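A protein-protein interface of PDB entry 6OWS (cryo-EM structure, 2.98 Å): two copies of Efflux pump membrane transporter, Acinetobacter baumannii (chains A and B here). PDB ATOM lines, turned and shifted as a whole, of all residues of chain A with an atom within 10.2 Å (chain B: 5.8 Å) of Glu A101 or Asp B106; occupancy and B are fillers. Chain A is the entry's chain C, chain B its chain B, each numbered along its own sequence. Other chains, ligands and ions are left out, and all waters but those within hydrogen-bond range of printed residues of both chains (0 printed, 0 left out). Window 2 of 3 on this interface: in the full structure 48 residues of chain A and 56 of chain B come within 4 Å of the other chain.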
ATOM      1  N   PRO A  41     -14.946  24.917  20.156  1.00  0.00           N
ATOM      2  CA  PRO A  41     -16.219  24.257  20.455  1.00  0.00           C
ATOM      3  C   PRO A  41     -16.739  24.587  21.841  1.00  0.00           C
ATOM      4  O   PRO A  41     -15.990  24.669  22.813  1.00  0.00           O
ATOM      5  CB  PRO A  41     -15.875  22.766  20.357  1.00  0.00           C
ATOM      6  CG  PRO A  41     -14.533  22.704  19.713  1.00  0.00           C
ATOM      7  CD  PRO A  41     -13.841  23.955  20.083  1.00  0.00           C
ATOM      8  N   GLN A  42     -18.054  24.753  21.920  1.00  0.00           N
ATOM      9  CA  GLN A  42     -18.742  25.072  23.159  1.00  0.00           C
ATOM     10  C   GLN A  42     -19.652  23.923  23.556  1.00  0.00           C
ATOM     11  O   GLN A  42     -20.218  23.242  22.703  1.00  0.00           O
ATOM     12  CB  GLN A  42     -19.577  26.338  23.019  1.00  0.00           C
ATOM     13  CG  GLN A  42     -18.782  27.605  22.870  1.00  0.00           C
ATOM     14  CD  GLN A  42     -19.653  28.829  22.973  1.00  0.00           C
ATOM     15  OE1 GLN A  42     -20.878  28.733  22.949  1.00  0.00           O
ATOM     16  NE2 GLN A  42     -19.029  29.994  23.084  1.00  0.00           N
ATOM     17  N   VAL A  43     -19.789  23.711  24.863  1.00  0.00           N
ATOM     18  CA  VAL A  43     -20.679  22.693  25.414  1.00  0.00           C
ATOM     19  C   VAL A  43     -21.518  23.351  26.496  1.00  0.00           C
ATOM     20  O   VAL A  43     -20.994  23.718  27.550  1.00  0.00           O
ATOM     21  CB  VAL A  43     -19.912  21.489  25.991  1.00  0.00           C
ATOM     22  CG1 VAL A  43     -20.875  20.504  26.604  1.00  0.00           C
ATOM     23  CG2 VAL A  43     -19.091  20.793  24.920  1.00  0.00           C
ATOM     24  N   VAL A  72     -11.401  19.455  33.357  1.00  0.00           N
ATOM     25  CA  VAL A  72     -11.683  18.919  32.037  1.00  0.00           C
ATOM     26  C   VAL A  72     -10.564  19.323  31.092  1.00  0.00           C
ATOM     27  O   VAL A  72     -10.218  20.507  30.982  1.00  0.00           O
ATOM     28  CB  VAL A  72     -13.045  19.422  31.540  1.00  0.00           C
ATOM     29  CG1 VAL A  72     -13.383  18.784  30.241  1.00  0.00           C
ATOM     30  CG2 VAL A  72     -14.112  19.101  32.550  1.00  0.00           C
ATOM     31  N   LYS A  73      -9.984  18.342  30.409  1.00  0.00           N
ATOM     32  CA  LYS A  73      -8.811  18.626  29.600  1.00  0.00           C
ATOM     33  C   LYS A  73      -9.199  19.332  28.307  1.00  0.00           C
ATOM     34  O   LYS A  73     -10.371  19.369  27.918  1.00  0.00           O
ATOM     35  CB  LYS A  73      -8.031  17.344  29.314  1.00  0.00           C
ATOM     36  CG  LYS A  73      -8.837  16.209  28.731  1.00  0.00           C
ATOM     37  CD  LYS A  73      -7.919  15.085  28.282  1.00  0.00           C
ATOM     38  CE  LYS A  73      -8.049  13.864  29.182  1.00  0.00           C
ATOM     39  NZ  LYS A  73      -9.358  13.162  29.029  1.00  0.00           N
ATOM     40  N   PHE A  94     -13.599  24.847  24.553  1.00  0.00           N
ATOM     41  CA  PHE A  94     -12.436  23.985  24.430  1.00  0.00           C
ATOM     42  C   PHE A  94     -11.462  24.536  23.401  1.00  0.00           C
ATOM     43  O   PHE A  94     -11.692  25.575  22.794  1.00  0.00           O
ATOM     44  CB  PHE A  94     -12.864  22.567  24.065  1.00  0.00           C
ATOM     45  CG  PHE A  94     -13.596  21.880  25.157  1.00  0.00           C
ATOM     46  CD1 PHE A  94     -12.905  21.234  26.158  1.00  0.00           C
ATOM     47  CD2 PHE A  94     -14.973  21.904  25.205  1.00  0.00           C
ATOM     48  CE1 PHE A  94     -13.568  20.612  27.173  1.00  0.00           C
ATOM     49  CE2 PHE A  94     -15.647  21.280  26.224  1.00  0.00           C
ATOM     50  CZ  PHE A  94     -14.940  20.633  27.211  1.00  0.00           C
ATOM     51  N   LYS A  95     -10.355  23.846  23.234  1.00  0.00           N
ATOM     52  CA  LYS A  95      -9.353  24.320  22.296  1.00  0.00           C
ATOM     53  C   LYS A  95      -9.765  23.990  20.865  1.00  0.00           C
ATOM     54  O   LYS A  95     -10.454  22.994  20.632  1.00  0.00           O
ATOM     55  CB  LYS A  95      -8.000  23.694  22.605  1.00  0.00           C
ATOM     56  CG  LYS A  95      -7.419  24.140  23.923  1.00  0.00           C
ATOM     57  CD  LYS A  95      -5.935  23.859  23.992  1.00  0.00           C
ATOM     58  CE  LYS A  95      -5.638  22.381  23.842  1.00  0.00           C
ATOM     59  NZ  LYS A  95      -4.196  22.141  23.570  1.00  0.00           N
ATOM     60  N   GLY A  97      -9.786  22.329  17.558  1.00  0.00           N
ATOM     61  CA  GLY A  97      -9.253  21.048  17.151  1.00  0.00           C
ATOM     62  C   GLY A  97      -9.663  19.902  18.042  1.00  0.00           C
ATOM     63  O   GLY A  97      -9.508  18.742  17.643  1.00  0.00           O
ATOM     64  N   THR A  98     -10.175  20.191  19.234  1.00  0.00           N
ATOM     65  CA  THR A  98     -10.660  19.157  20.134  1.00  0.00           C
ATOM     66  C   THR A  98     -11.916  18.509  19.560  1.00  0.00           C
ATOM     67  O   THR A  98     -12.793  19.196  19.034  1.00  0.00           O
ATOM     68  CB  THR A  98     -10.939  19.772  21.508  1.00  0.00           C
ATOM     69  OG1 THR A  98      -9.722  20.312  22.035  1.00  0.00           O
ATOM     70  CG2 THR A  98     -11.483  18.754  22.490  1.00  0.00           C
ATOM     71  N   ASP A  99     -11.979  17.178  19.625  1.00  0.00           N
ATOM     72  CA  ASP A  99     -13.129  16.447  19.110  1.00  0.00           C
ATOM     73  C   ASP A  99     -14.340  16.733  19.988  1.00  0.00           C
ATOM     74  O   ASP A  99     -14.290  16.548  21.208  1.00  0.00           O
ATOM     75  CB  ASP A  99     -12.823  14.952  19.060  1.00  0.00           C
ATOM     76  CG  ASP A  99     -13.857  14.154  18.266  1.00  0.00           C
ATOM     77  OD1 ASP A  99     -15.043  14.099  18.658  1.00  0.00           O
ATOM     78  OD2 ASP A  99     -13.474  13.576  17.227  1.00  0.00           O
ATOM     79  N   VAL A 100     -15.432  17.167  19.358  1.00  0.00           N
ATOM     80  CA  VAL A 100     -16.552  17.740  20.088  1.00  0.00           C
ATOM     81  C   VAL A 100     -17.366  16.698  20.839  1.00  0.00           C
ATOM     82  O   VAL A 100     -18.127  17.056  21.743  1.00  0.00           O
ATOM     83  CB  VAL A 100     -17.458  18.530  19.128  1.00  0.00           C
ATOM     84  CG1 VAL A 100     -16.675  19.640  18.464  1.00  0.00           C
ATOM     85  CG2 VAL A 100     -18.056  17.611  18.081  1.00  0.00           C
ATOM     86  N   GLU A 101     -17.243  15.418  20.497  1.00  0.00           N
ATOM     87  CA  GLU A 101     -18.000  14.422  21.240  1.00  0.00           C
ATOM     88  C   GLU A 101     -17.210  13.848  22.403  1.00  0.00           C
ATOM     89  O   GLU A 101     -17.749  13.699  23.505  1.00  0.00           O
ATOM     90  CB  GLU A 101     -18.473  13.303  20.314  1.00  0.00           C
ATOM     91  CG  GLU A 101     -19.245  12.230  21.054  1.00  0.00           C
ATOM     92  CD  GLU A 101     -20.732  12.486  21.071  1.00  0.00           C
ATOM     93  OE1 GLU A 101     -21.220  13.252  20.214  1.00  0.00           O
ATOM     94  OE2 GLU A 101     -21.414  11.934  21.959  1.00  0.00           O
ATOM     95  N   MET A 102     -15.924  13.566  22.197  1.00  0.00           N
ATOM     96  CA  MET A 102     -15.093  13.079  23.290  1.00  0.00           C
ATOM     97  C   MET A 102     -14.793  14.160  24.317  1.00  0.00           C
ATOM     98  O   MET A 102     -14.304  13.842  25.405  1.00  0.00           O
ATOM     99  CB  MET A 102     -13.788  12.504  22.745  1.00  0.00           C
ATOM    100  CG  MET A 102     -13.928  11.113  22.150  1.00  0.00           C
ATOM    101  SD  MET A 102     -14.666   9.913  23.276  1.00  0.00           S
ATOM    102  CE  MET A 102     -13.483   9.917  24.612  1.00  0.00           C
ATOM    103  N   ALA A 103     -15.073  15.423  23.998  1.00  0.00           N
ATOM    104  CA  ALA A 103     -15.107  16.471  25.002  1.00  0.00           C
ATOM    105  C   ALA A 103     -16.460  16.566  25.683  1.00  0.00           C
ATOM    106  O   ALA A 103     -16.532  17.019  26.827  1.00  0.00           O
ATOM    107  CB  ALA A 103     -14.751  17.813  24.371  1.00  0.00           C
ATOM    108  N   GLN A 104     -17.530  16.152  25.011  1.00  0.00           N
ATOM    109  CA  GLN A 104     -18.841  16.147  25.639  1.00  0.00           C
ATOM    110  C   GLN A 104     -18.987  15.024  26.650  1.00  0.00           C
ATOM    111  O   GLN A 104     -19.724  15.176  27.627  1.00  0.00           O
ATOM    112  CB  GLN A 104     -19.939  16.027  24.583  1.00  0.00           C
ATOM    113  CG  GLN A 104     -21.310  16.423  25.089  1.00  0.00           C
ATOM    114  CD  GLN A 104     -22.361  16.432  24.010  1.00  0.00           C
ATOM    115  OE1 GLN A 104     -22.051  16.487  22.824  1.00  0.00           O
ATOM    116  NE2 GLN A 104     -23.621  16.378  24.418  1.00  0.00           N
ATOM    117  N   VAL A 105     -18.288  13.907  26.453  1.00  0.00           N
ATOM    118  CA  VAL A 105     -18.354  12.836  27.437  1.00  0.00           C
ATOM    119  C   VAL A 105     -17.534  13.157  28.676  1.00  0.00           C
ATOM    120  O   VAL A 105     -17.755  12.542  29.720  1.00  0.00           O
ATOM    121  CB  VAL A 105     -17.910  11.498  26.827  1.00  0.00           C
ATOM    122  CG1 VAL A 105     -18.712  11.203  25.584  1.00  0.00           C
ATOM    123  CG2 VAL A 105     -16.437  11.524  26.494  1.00  0.00           C
ATOM    124  N   ASP A 106     -16.604  14.111  28.594  1.00  0.00           N
ATOM    125  CA  ASP A 106     -15.879  14.542  29.783  1.00  0.00           C
ATOM    126  C   ASP A 106     -16.792  15.269  30.752  1.00  0.00           C
ATOM    127  O   ASP A 106     -16.748  15.014  31.958  1.00  0.00           O
ATOM    128  CB  ASP A 106     -14.715  15.447  29.398  1.00  0.00           C
ATOM    129  CG  ASP A 106     -13.570  14.691  28.783  1.00  0.00           C
ATOM    130  OD1 ASP A 106     -13.373  13.517  29.139  1.00  0.00           O
ATOM    131  OD2 ASP A 106     -12.857  15.275  27.940  1.00  0.00           O
ATOM    132  N   VAL A 107     -17.618  16.187  30.247  1.00  0.00           N
ATOM    133  CA  VAL A 107     -18.486  16.927  31.150  1.00  0.00           C
ATOM    134  C   VAL A 107     -19.625  16.050  31.641  1.00  0.00           C
ATOM    135  O   VAL A 107     -20.090  16.227  32.764  1.00  0.00           O
ATOM    136  CB  VAL A 107     -18.979  18.233  30.495  1.00  0.00           C
ATOM    137  CG1 VAL A 107     -17.801  19.058  30.044  1.00  0.00           C
ATOM    138  CG2 VAL A 107     -19.876  17.968  29.320  1.00  0.00           C
ATOM    139  N   GLN A 108     -20.047  15.051  30.858  1.00  0.00           N
ATOM    140  CA  GLN A 108     -21.067  14.126  31.340  1.00  0.00           C
ATOM    141  C   GLN A 108     -20.557  13.253  32.479  1.00  0.00           C
ATOM    142  O   GLN A 108     -21.361  12.780  33.288  1.00  0.00           O
ATOM    143  CB  GLN A 108     -21.575  13.251  30.196  1.00  0.00           C
ATOM    144  CG  GLN A 108     -22.388  13.989  29.157  1.00  0.00           C
ATOM    145  CD  GLN A 108     -23.873  13.907  29.421  1.00  0.00           C
ATOM    146  OE1 GLN A 108     -24.308  13.843  30.568  1.00  0.00           O
ATOM    147  NE2 GLN A 108     -24.664  13.914  28.356  1.00  0.00           N
ATOM    148  N   ASN A 109     -19.241  13.048  32.564  1.00  0.00           N
ATOM    149  CA  ASN A 109     -18.660  12.333  33.692  1.00  0.00           C
ATOM    150  C   ASN A 109     -18.802  13.121  34.986  1.00  0.00           C
ATOM    151  O   ASN A 109     -19.013  12.538  36.054  1.00  0.00           O
ATOM    152  CB  ASN A 109     -17.184  12.043  33.427  1.00  0.00           C
ATOM    153  CG  ASN A 109     -16.972  11.042  32.318  1.00  0.00           C
ATOM    154  OD1 ASN A 109     -17.923  10.474  31.784  1.00  0.00           O
ATOM    155  ND2 ASN A 109     -15.716  10.827  31.954  1.00  0.00           N
ATOM    156  N   VAL A 129     -27.241  18.645  28.765  1.00  0.00           N
ATOM    157  CA  VAL A 129     -25.896  18.933  28.287  1.00  0.00           C
ATOM    158  C   VAL A 129     -25.931  18.799  26.776  1.00  0.00           C
ATOM    159  O   VAL A 129     -26.179  17.706  26.254  1.00  0.00           O
ATOM    160  CB  VAL A 129     -24.841  17.990  28.878  1.00  0.00           C
ATOM    161  CG1 VAL A 129     -23.466  18.411  28.425  1.00  0.00           C
ATOM    162  CG2 VAL A 129     -24.923  17.968  30.374  1.00  0.00           C
ATOM    163  N   GLU A 130     -25.695  19.898  26.073  1.00  0.00           N
ATOM    164  CA  GLU A 130     -25.864  19.910  24.632  1.00  0.00           C
ATOM    165  C   GLU A 130     -24.899  20.915  24.025  1.00  0.00           C
ATOM    166  O   GLU A 130     -24.839  22.071  24.443  1.00  0.00           O
ATOM    167  CB  GLU A 130     -27.323  20.224  24.288  1.00  0.00           C
ATOM    168  CG  GLU A 130     -27.715  19.974  22.850  1.00  0.00           C
ATOM    169  CD  GLU A 130     -27.527  21.188  21.980  1.00  0.00           C
ATOM    170  OE1 GLU A 130     -27.626  22.309  22.520  1.00  0.00           O
ATOM    171  OE2 GLU A 130     -27.289  21.025  20.766  1.00  0.00           O
ATOM    172  N   ALA A 131     -24.137  20.459  23.037  1.00  0.00           N
ATOM    173  CA  ALA A 131     -23.099  21.263  22.401  1.00  0.00           C
ATOM    174  C   ALA A 131     -23.673  21.902  21.145  1.00  0.00           C
ATOM    175  O   ALA A 131     -23.840  21.230  20.125  1.00  0.00           O
ATOM    176  CB  ALA A 131     -21.884  20.404  22.064  1.00  0.00           C
ATOM    177  N   SER A 294     -26.589  21.762  13.775  1.00  0.00           N
ATOM    178  CA  SER A 294     -25.867  20.869  14.659  1.00  0.00           C
ATOM    179  C   SER A 294     -24.357  21.097  14.573  1.00  0.00           C
ATOM    180  O   SER A 294     -23.868  21.734  13.637  1.00  0.00           O
ATOM    181  CB  SER A 294     -26.202  19.423  14.301  1.00  0.00           C
ATOM    182  OG  SER A 294     -27.579  19.172  14.459  1.00  0.00           O
ATOM    183  N   PRO A 295     -23.598  20.610  15.554  1.00  0.00           N
ATOM    184  CA  PRO A 295     -22.143  20.561  15.387  1.00  0.00           C
ATOM    185  C   PRO A 295     -21.749  19.544  14.329  1.00  0.00           C
ATOM    186  O   PRO A 295     -22.209  18.402  14.338  1.00  0.00           O
ATOM    187  CB  PRO A 295     -21.640  20.149  16.776  1.00  0.00           C
ATOM    188  CG  PRO A 295     -22.821  19.514  17.432  1.00  0.00           C
ATOM    189  CD  PRO A 295     -23.978  20.314  16.947  1.00  0.00           C
ATOM    190  N   GLY A 296     -20.877  19.967  13.419  1.00  0.00           N
ATOM    191  CA  GLY A 296     -20.508  19.123  12.302  1.00  0.00           C
ATOM    192  C   GLY A 296     -21.657  18.955  11.334  1.00  0.00           C
ATOM    193  O   GLY A 296     -22.067  17.832  11.028  1.00  0.00           O
ATOM    194  N   VAL B  72     -28.620  11.800  15.037  1.00  0.00           N
ATOM    195  CA  VAL B  72     -27.484  10.950  15.361  1.00  0.00           C
ATOM    196  C   VAL B  72     -26.769  10.571  14.075  1.00  0.00           C
ATOM    197  O   VAL B  72     -27.387  10.074  13.124  1.00  0.00           O
ATOM    198  CB  VAL B  72     -27.956   9.706  16.126  1.00  0.00           C
ATOM    199  CG1 VAL B  72     -26.784   8.897  16.556  1.00  0.00           C
ATOM    200  CG2 VAL B  72     -28.752  10.115  17.334  1.00  0.00           C
ATOM    201  N   LYS B  73     -25.463  10.810  14.032  1.00  0.00           N
ATOM    202  CA  LYS B  73     -24.737  10.618  12.789  1.00  0.00           C
ATOM    203  C   LYS B  73     -24.501   9.137  12.522  1.00  0.00           C
ATOM    204  O   LYS B  73     -24.662   8.287  13.403  1.00  0.00           O
ATOM    205  CB  LYS B  73     -23.421  11.392  12.808  1.00  0.00           C
ATOM    206  CG  LYS B  73     -22.536  11.137  14.005  1.00  0.00           C
ATOM    207  CD  LYS B  73     -21.173  11.777  13.801  1.00  0.00           C
ATOM    208  CE  LYS B  73     -20.975  12.978  14.716  1.00  0.00           C
ATOM    209  NZ  LYS B  73     -20.832  12.598  16.153  1.00  0.00           N
ATOM    210  N   PHE B  94     -27.255   1.636  12.531  1.00  0.00           N
ATOM    211  CA  PHE B  94     -26.204   2.503  12.029  1.00  0.00           C
ATOM    212  C   PHE B  94     -25.581   1.925  10.770  1.00  0.00           C
ATOM    213  O   PHE B  94     -25.967   0.861  10.295  1.00  0.00           O
ATOM    214  CB  PHE B  94     -25.143   2.723  13.105  1.00  0.00           C
ATOM    215  CG  PHE B  94     -25.635   3.527  14.252  1.00  0.00           C
ATOM    216  CD1 PHE B  94     -25.620   4.903  14.192  1.00  0.00           C
ATOM    217  CD2 PHE B  94     -26.141   2.913  15.378  1.00  0.00           C
ATOM    218  CE1 PHE B  94     -26.083   5.651  15.234  1.00  0.00           C
ATOM    219  CE2 PHE B  94     -26.607   3.659  16.429  1.00  0.00           C
ATOM    220  CZ  PHE B  94     -26.577   5.032  16.356  1.00  0.00           C
ATOM    221  N   GLU B 101     -19.408   1.527  20.084  1.00  0.00           N
ATOM    222  CA  GLU B 101     -19.468   2.210  21.367  1.00  0.00           C
ATOM    223  C   GLU B 101     -19.577   3.717  21.210  1.00  0.00           C
ATOM    224  O   GLU B 101     -20.376   4.357  21.903  1.00  0.00           O
ATOM    225  CB  GLU B 101     -18.259   1.850  22.229  1.00  0.00           C
ATOM    226  CG  GLU B 101     -18.271   2.562  23.565  1.00  0.00           C
ATOM    227  CD  GLU B 101     -18.951   1.760  24.648  1.00  0.00           C
ATOM    228  OE1 GLU B 101     -19.074   0.529  24.496  1.00  0.00           O
ATOM    229  OE2 GLU B 101     -19.383   2.371  25.648  1.00  0.00           O
ATOM    230  N   MET B 102     -18.823   4.299  20.277  1.00  0.00           N
ATOM    231  CA  MET B 102     -18.930   5.729  20.030  1.00  0.00           C
ATOM    232  C   MET B 102     -20.238   6.105  19.347  1.00  0.00           C
ATOM    233  O   MET B 102     -20.570   7.292  19.287  1.00  0.00           O
ATOM    234  CB  MET B 102     -17.749   6.211  19.191  1.00  0.00           C
ATOM    235  CG  MET B 102     -16.462   6.382  19.978  1.00  0.00           C
ATOM    236  SD  MET B 102     -16.628   7.457  21.418  1.00  0.00           S
ATOM    237  CE  MET B 102     -17.112   8.994  20.648  1.00  0.00           C
ATOM    238  N   ALA B 103     -20.980   5.123  18.834  1.00  0.00           N
ATOM    239  CA  ALA B 103     -22.360   5.343  18.440  1.00  0.00           C
ATOM    240  C   ALA B 103     -23.320   5.174  19.604  1.00  0.00           C
ATOM    241  O   ALA B 103     -24.399   5.769  19.590  1.00  0.00           O
ATOM    242  CB  ALA B 103     -22.741   4.387  17.315  1.00  0.00           C
ATOM    243  N   GLN B 104     -22.954   4.382  20.608  1.00  0.00           N
ATOM    244  CA  GLN B 104     -23.797   4.241  21.783  1.00  0.00           C
ATOM    245  C   GLN B 104     -23.744   5.467  22.674  1.00  0.00           C
ATOM    246  O   GLN B 104     -24.731   5.777  23.346  1.00  0.00           O
ATOM    247  CB  GLN B 104     -23.390   3.008  22.589  1.00  0.00           C
ATOM    248  CG  GLN B 104     -24.447   2.555  23.575  1.00  0.00           C
ATOM    249  CD  GLN B 104     -24.098   1.265  24.269  1.00  0.00           C
ATOM    250  OE1 GLN B 104     -23.255   0.502  23.802  1.00  0.00           O
ATOM    251  NE2 GLN B 104     -24.747   1.009  25.395  1.00  0.00           N
ATOM    252  N   VAL B 105     -22.624   6.190  22.683  1.00  0.00           N
ATOM    253  CA  VAL B 105     -22.563   7.409  23.476  1.00  0.00           C
ATOM    254  C   VAL B 105     -23.318   8.549  22.818  1.00  0.00           C
ATOM    255  O   VAL B 105     -23.657   9.521  23.498  1.00  0.00           O
ATOM    256  CB  VAL B 105     -21.105   7.814  23.753  1.00  0.00           C
ATOM    257  CG1 VAL B 105     -20.360   6.663  24.384  1.00  0.00           C
ATOM    258  CG2 VAL B 105     -20.417   8.238  22.479  1.00  0.00           C
ATOM    259  N   ASP B 106     -23.602   8.458  21.516  1.00  0.00           N
ATOM    260  CA  ASP B 106     -24.432   9.464  20.866  1.00  0.00           C
ATOM    261  C   ASP B 106     -25.864   9.405  21.365  1.00  0.00           C
ATOM    262  O   ASP B 106     -26.466  10.443  21.655  1.00  0.00           O
ATOM    263  CB  ASP B 106     -24.409   9.279  19.354  1.00  0.00           C
ATOM    264  CG  ASP B 106     -23.112   9.721  18.734  1.00  0.00           C
ATOM    265  OD1 ASP B 106     -22.482  10.648  19.273  1.00  0.00           O
ATOM    266  OD2 ASP B 106     -22.720   9.143  17.699  1.00  0.00           O
ATOM    267  N   VAL B 107     -26.432   8.203  21.462  1.00  0.00           N
ATOM    268  CA  VAL B 107     -27.814   8.109  21.905  1.00  0.00           C
ATOM    269  C   VAL B 107     -27.918   8.371  23.400  1.00  0.00           C
ATOM    270  O   VAL B 107     -28.927   8.903  23.857  1.00  0.00           O
ATOM    271  CB  VAL B 107     -28.438   6.760  21.494  1.00  0.00           C
ATOM    272  CG1 VAL B 107     -28.311   6.570  20.005  1.00  0.00           C
ATOM    273  CG2 VAL B 107     -27.787   5.602  22.197  1.00  0.00           C
ATOM    274  N   GLN B 108     -26.868   8.083  24.175  1.00  0.00           N
ATOM    275  CA  GLN B 108     -26.893   8.416  25.594  1.00  0.00           C
ATOM    276  C   GLN B 108     -26.875   9.920  25.831  1.00  0.00           C
ATOM    277  O   GLN B 108     -27.351  10.376  26.875  1.00  0.00           O
ATOM    278  CB  GLN B 108     -25.718   7.759  26.319  1.00  0.00           C
ATOM    279  CG  GLN B 108     -25.811   6.254  26.421  1.00  0.00           C
ATOM    280  CD  GLN B 108     -26.421   5.799  27.726  1.00  0.00           C
ATOM    281  OE1 GLN B 108     -27.273   6.479  28.294  1.00  0.00           O
ATOM    282  NE2 GLN B 108     -25.992   4.641  28.208  1.00  0.00           N
ATOM    283  N   ASN B 109     -26.355  10.692  24.875  1.00  0.00           N
ATOM    284  CA  ASN B 109     -26.412  12.146  24.964  1.00  0.00           C
ATOM    285  C   ASN B 109     -27.841  12.654  24.845  1.00  0.00           C
ATOM    286  O   ASN B 109     -28.215  13.632  25.503  1.00  0.00           O
ATOM    287  CB  ASN B 109     -25.552  12.774  23.870  1.00  0.00           C
ATOM    288  CG  ASN B 109     -24.075  12.537  24.076  1.00  0.00           C
ATOM    289  OD1 ASN B 109     -23.656  11.977  25.088  1.00  0.00           O
ATOM    290  ND2 ASN B 109     -23.274  12.955  23.107  1.00  0.00           N
ATOM    291  N   LYS B 110     -28.655  12.013  24.012  1.00  0.00           N
ATOM    292  CA  LYS B 110     -29.899  12.627  23.571  1.00  0.00           C
ATOM    293  C   LYS B 110     -31.108  12.312  24.440  1.00  0.00           C
ATOM    294  O   LYS B 110     -31.945  13.195  24.638  1.00  0.00           O
ATOM    295  CB  LYS B 110     -30.193  12.218  22.130  1.00  0.00           C
ATOM    296  CG  LYS B 110     -29.718  13.224  21.100  1.00  0.00           C
ATOM    297  CD  LYS B 110     -28.275  13.004  20.715  1.00  0.00           C
ATOM    298  CE  LYS B 110     -27.895  13.837  19.506  1.00  0.00           C
ATOM    299  NZ  LYS B 110     -26.435  13.760  19.215  1.00  0.00           N
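The side-chain amide nitrogen (ND2) of Asn B109 is in hydrogen-bond range of the side-chain carboxylate (OE2) of Glu A101, at 2.4 Å.
The side-chain carboxylate of Glu A101 sits close to the side-chain carboxylate of Asp B106 (3.0 Å).
The side-chain sulfur (SD) of Met A102 sits close to the side-chain sulfur (SD) of Met B102.
O of Val B105 sits close to OD1 of Asn B109.
OD1 of Asp A99 lies within hydrogen-bond range of N of Glu A101 (3.2 Å).
The backbone carbonyl oxygen (O) of Val A129 lies within hydrogen-bond range of the side-chain amide nitrogen (NE2) of Gln A104.
Glu A101 touches four residues of chain B.
Printed residues of chain B within 4 Å of Met A102: Met B102 (3.7 Å).
Of the printed residues of chain B, Gln A104 touches Asn B109.
Printed residues of chain B within 4 Å of Gln A108: Asn B109.
No residue of chain A comes within 4 Å of Lys B73.
Printed residues of chain A within 4 Å of Met B102: Glu A101 and Met A102.
No residue of chain A comes within 4 Å of Ala B103.
Val B105 touches just one residue of chain A: Glu A101 (3.6 Å).
Asp B106 touches just one residue of chain A: Glu A101 (3.0 Å).
The nearest residue of chain B that does not touch Glu A101 is Lys B73 (4.1 Å).
CG of Glu A101 touches CE of Met B102, 3.9 Å away.
Glu A101 touches Val B105.
ND2 of Asn B109 touches NE2 of Gln A104 (3.7 Å).
Gln A108 touches Asn B109.
Hydrophobic or aromatic side chains of chain B that line the printed part of chain A: Met B102 and Val B105.
Hydrophobic or aromatic side chains of chain A within 4 Å of the printed part of chain B: Met A102.
Along chain A the printed residues that touch a printed residue of chain B span positions 101 to 108.
Glu A101 touches Met B102, but with the chains exchanged Met A102 does not touch Glu B101 (8.1 Å).
Glu A101 touches Val B105, but with the chains exchanged Val A105 does not touch Glu B101 (7.9 Å).
Met B102 touches its own counterpart, Met A102.
Gln A108 touches Asn B109, but with the chains exchanged Asn A109 does not touch Gln B108 (9.9 Å).
Positions printed for both chains: 72, 73, 94, 101, 102, 103, 104, 105, 106, 107, 108 and 109.
Of the 7 pairs that touch across the chains among the printed residues, 1 has its exchanged pair printed and touching as well.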
